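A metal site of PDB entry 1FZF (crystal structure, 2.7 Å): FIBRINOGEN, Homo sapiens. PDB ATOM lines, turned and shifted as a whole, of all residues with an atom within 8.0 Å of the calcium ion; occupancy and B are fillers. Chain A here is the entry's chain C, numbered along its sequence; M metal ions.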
ATOM      1  N   SER A 226      -7.534  28.456  -7.623  1.00  0.00           N
ATOM      2  CA  SER A 226      -6.338  28.049  -8.354  1.00  0.00           C
ATOM      3  C   SER A 226      -6.464  26.669  -9.012  1.00  0.00           C
ATOM      4  O   SER A 226      -7.068  25.762  -8.446  1.00  0.00           O
ATOM      5  CB  SER A 226      -5.116  28.033  -7.425  1.00  0.00           C
ATOM      6  OG  SER A 226      -4.716  29.333  -7.047  1.00  0.00           O
ATOM      7  N   ASN A 230      -3.483  27.594 -13.695  1.00  0.00           N
ATOM      8  CA  ASN A 230      -3.749  28.963 -13.261  1.00  0.00           C
ATOM      9  C   ASN A 230      -3.468  29.143 -11.765  1.00  0.00           C
ATOM     10  O   ASN A 230      -4.379  29.168 -10.933  1.00  0.00           O
ATOM     11  CB  ASN A 230      -5.198  29.348 -13.579  1.00  0.00           C
ATOM     12  CG  ASN A 230      -5.380  30.839 -13.791  1.00  0.00           C
ATOM     13  OD1 ASN A 230      -6.018  31.259 -14.759  1.00  0.00           O
ATOM     14  ND2 ASN A 230      -4.812  31.649 -12.899  1.00  0.00           N
ATOM     15  N   ASP A 231      -2.173  29.305 -11.446  1.00  0.00           N
ATOM     16  CA  ASP A 231      -1.653  29.464 -10.076  1.00  0.00           C
ATOM     17  C   ASP A 231      -1.948  30.842  -9.489  1.00  0.00           C
ATOM     18  O   ASP A 231      -1.414  31.851  -9.951  1.00  0.00           O
ATOM     19  CB  ASP A 231      -0.139  29.209 -10.088  1.00  0.00           C
ATOM     20  CG  ASP A 231       0.476  29.094  -8.695  1.00  0.00           C
ATOM     21  OD1 ASP A 231      -0.137  29.549  -7.708  1.00  0.00           O
ATOM     22  OD2 ASP A 231       1.605  28.549  -8.581  1.00  0.00           O
ATOM     23  N   ASN A 232      -2.783  30.874  -8.450  1.00  0.00           N
ATOM     24  CA  ASN A 232      -3.141  32.117  -7.772  1.00  0.00           C
ATOM     25  C   ASN A 232      -3.013  31.979  -6.256  1.00  0.00           C
ATOM     26  O   ASN A 232      -3.633  32.736  -5.509  1.00  0.00           O
ATOM     27  CB  ASN A 232      -4.571  32.521  -8.121  1.00  0.00           C
ATOM     28  CG  ASN A 232      -4.726  32.923  -9.564  1.00  0.00           C
ATOM     29  OD1 ASN A 232      -5.597  32.411 -10.272  1.00  0.00           O
ATOM     30  ND2 ASN A 232      -3.890  33.847 -10.016  1.00  0.00           N
ATOM     31  N   ASP A 233      -2.228  31.008  -5.806  1.00  0.00           N
ATOM     32  CA  ASP A 233      -2.039  30.802  -4.379  1.00  0.00           C
ATOM     33  C   ASP A 233      -0.955  31.707  -3.813  1.00  0.00           C
ATOM     34  O   ASP A 233      -0.263  32.409  -4.574  1.00  0.00           O
ATOM     35  CB  ASP A 233      -1.717  29.325  -4.068  1.00  0.00           C
ATOM     36  CG  ASP A 233      -0.479  28.817  -4.771  1.00  0.00           C
ATOM     37  OD1 ASP A 233       0.385  29.617  -5.198  1.00  0.00           O
ATOM     38  OD2 ASP A 233      -0.355  27.588  -4.885  1.00  0.00           O
ATOM     39  N   LYS A 234      -0.817  31.676  -2.494  1.00  0.00           N
ATOM     40  CA  LYS A 234       0.184  32.491  -1.791  1.00  0.00           C
ATOM     41  C   LYS A 234       1.390  31.599  -1.494  1.00  0.00           C
ATOM     42  O   LYS A 234       2.004  31.682  -0.430  1.00  0.00           O
ATOM     43  CB  LYS A 234      -0.406  33.028  -0.476  1.00  0.00           C
ATOM     44  CG  LYS A 234      -1.765  33.718  -0.611  1.00  0.00           C
ATOM     45  CD  LYS A 234      -1.739  34.966  -1.500  1.00  0.00           C
ATOM     46  CE  LYS A 234      -1.107  36.144  -0.786  1.00  0.00           C
ATOM     47  NZ  LYS A 234      -1.059  37.353  -1.664  1.00  0.00           N
ATOM     48  N   PHE A 235       1.739  30.774  -2.474  1.00  0.00           N
ATOM     49  CA  PHE A 235       2.848  29.844  -2.369  1.00  0.00           C
ATOM     50  C   PHE A 235       3.735  30.022  -3.579  1.00  0.00           C
ATOM     51  O   PHE A 235       3.250  30.121  -4.694  1.00  0.00           O
ATOM     52  CB  PHE A 235       2.259  28.430  -2.352  1.00  0.00           C
ATOM     53  CG  PHE A 235       3.268  27.340  -2.486  1.00  0.00           C
ATOM     54  CD1 PHE A 235       4.509  27.425  -1.855  1.00  0.00           C
ATOM     55  CD2 PHE A 235       2.959  26.190  -3.202  1.00  0.00           C
ATOM     56  CE1 PHE A 235       5.417  26.382  -1.939  1.00  0.00           C
ATOM     57  CE2 PHE A 235       3.865  25.141  -3.294  1.00  0.00           C
ATOM     58  CZ  PHE A 235       5.099  25.237  -2.657  1.00  0.00           C
ATOM     59  N   GLU A 236       5.051  30.059  -3.361  1.00  0.00           N
ATOM     60  CA  GLU A 236       6.021  30.221  -4.449  1.00  0.00           C
ATOM     61  C   GLU A 236       5.869  29.107  -5.469  1.00  0.00           C
ATOM     62  O   GLU A 236       6.213  29.274  -6.640  1.00  0.00           O
ATOM     63  CB  GLU A 236       7.462  30.287  -3.924  1.00  0.00           C
ATOM     64  CG  GLU A 236       7.731  29.521  -2.625  1.00  0.00           C
ATOM     65  CD  GLU A 236       7.160  30.212  -1.366  1.00  0.00           C
ATOM     66  OE1 GLU A 236       6.857  31.440  -1.403  1.00  0.00           O
ATOM     67  OE2 GLU A 236       7.029  29.527  -0.334  1.00  0.00           O
ATOM     68  N   GLY A 237       5.339  27.982  -5.009  1.00  0.00           N
ATOM     69  CA  GLY A 237       5.117  26.859  -5.893  1.00  0.00           C
ATOM     70  C   GLY A 237       3.663  26.838  -6.347  1.00  0.00           C
ATOM     71  O   GLY A 237       2.945  27.843  -6.212  1.00  0.00           O
ATOM     72  N   ASN A 238       3.217  25.685  -6.827  1.00  0.00           N
ATOM     73  CA  ASN A 238       1.862  25.535  -7.319  1.00  0.00           C
ATOM     74  C   ASN A 238       1.072  24.504  -6.503  1.00  0.00           C
ATOM     75  O   ASN A 238       1.113  23.302  -6.811  1.00  0.00           O
ATOM     76  CB  ASN A 238       1.915  25.128  -8.794  1.00  0.00           C
ATOM     77  CG  ASN A 238       0.567  25.200  -9.482  1.00  0.00           C
ATOM     78  OD1 ASN A 238       0.500  25.145 -10.713  1.00  0.00           O
ATOM     79  ND2 ASN A 238      -0.508  25.347  -8.707  1.00  0.00           N
ATOM     80  N   CYS A 239       0.337  24.981  -5.493  1.00  0.00           N
ATOM     81  CA  CYS A 239      -0.473  24.121  -4.612  1.00  0.00           C
ATOM     82  C   CYS A 239      -1.384  23.182  -5.407  1.00  0.00           C
ATOM     83  O   CYS A 239      -1.416  21.971  -5.143  1.00  0.00           O
ATOM     84  CB  CYS A 239      -1.342  24.968  -3.674  1.00  0.00           C
ATOM     85  SG  CYS A 239      -0.499  25.712  -2.232  1.00  0.00           S
ATOM     86  N   ALA A 240      -2.096  23.739  -6.374  1.00  0.00           N
ATOM     87  CA  ALA A 240      -3.020  22.979  -7.225  1.00  0.00           C
ATOM     88  C   ALA A 240      -2.359  21.867  -8.030  1.00  0.00           C
ATOM     89  O   ALA A 240      -2.887  20.756  -8.078  1.00  0.00           O
ATOM     90  CB  ALA A 240      -3.774  23.926  -8.147  1.00  0.00           C
ATOM     91  N   GLN A 242       0.487  20.505  -7.329  1.00  0.00           N
ATOM     92  CA  GLN A 242       1.041  19.583  -6.345  1.00  0.00           C
ATOM     93  C   GLN A 242       0.047  18.682  -5.646  1.00  0.00           C
ATOM     94  O   GLN A 242       0.396  17.585  -5.209  1.00  0.00           O
ATOM     95  CB  GLN A 242       1.864  20.338  -5.314  1.00  0.00           C
ATOM     96  CG  GLN A 242       3.160  20.875  -5.879  1.00  0.00           C
ATOM     97  CD  GLN A 242       3.882  21.776  -4.912  1.00  0.00           C
ATOM     98  OE1 GLN A 242       4.117  21.402  -3.762  1.00  0.00           O
ATOM     99  NE2 GLN A 242       4.234  22.981  -5.368  1.00  0.00           N
ATOM    100  N   LYS A 251      -0.975  29.049   0.171  1.00  0.00           N
ATOM    101  CA  LYS A 251       0.210  28.311   0.648  1.00  0.00           C
ATOM    102  C   LYS A 251      -0.315  26.966   1.147  1.00  0.00           C
ATOM    103  O   LYS A 251       0.013  26.444   2.235  1.00  0.00           O
ATOM    104  CB  LYS A 251       1.012  29.046   1.724  1.00  0.00           C
ATOM    105  CG  LYS A 251       2.470  28.622   1.738  1.00  0.00           C
ATOM    106  CD  LYS A 251       3.388  29.778   2.111  1.00  0.00           C
ATOM    107  CE  LYS A 251       4.858  29.380   2.027  1.00  0.00           C
ATOM    108  NZ  LYS A 251       5.773  30.542   2.269  1.00  0.00           N
HETATM  109 CA    CA M   1       2.168  30.243  -6.779  1.00  0.00          CA
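OD2 of Asp 233 sits at hydrogen-bond distance from N of Cys 239, 2.8 Å away.
The backbone NH of Asp 233 lies within hydrogen-bond range of the side-chain hydroxyl of Ser 226 (3.2 Å).
Of the 14 residues printed, 4 come within 4 Å of the calcium ion.
O of Phe 235 is bound to the calcium ion, 2.4 Å away.
OD1 of Asp 233 is bound to the calcium ion (2.5 Å).
The calcium ion is bound by the side-chain carboxylate (OD2) of Asp 231 (2.5 Å).
OD1 of Asp 231 is bound to the calcium ion (2.6 Å).
The calcium ion is bound by O of Gly 237, 2.6 Å away.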
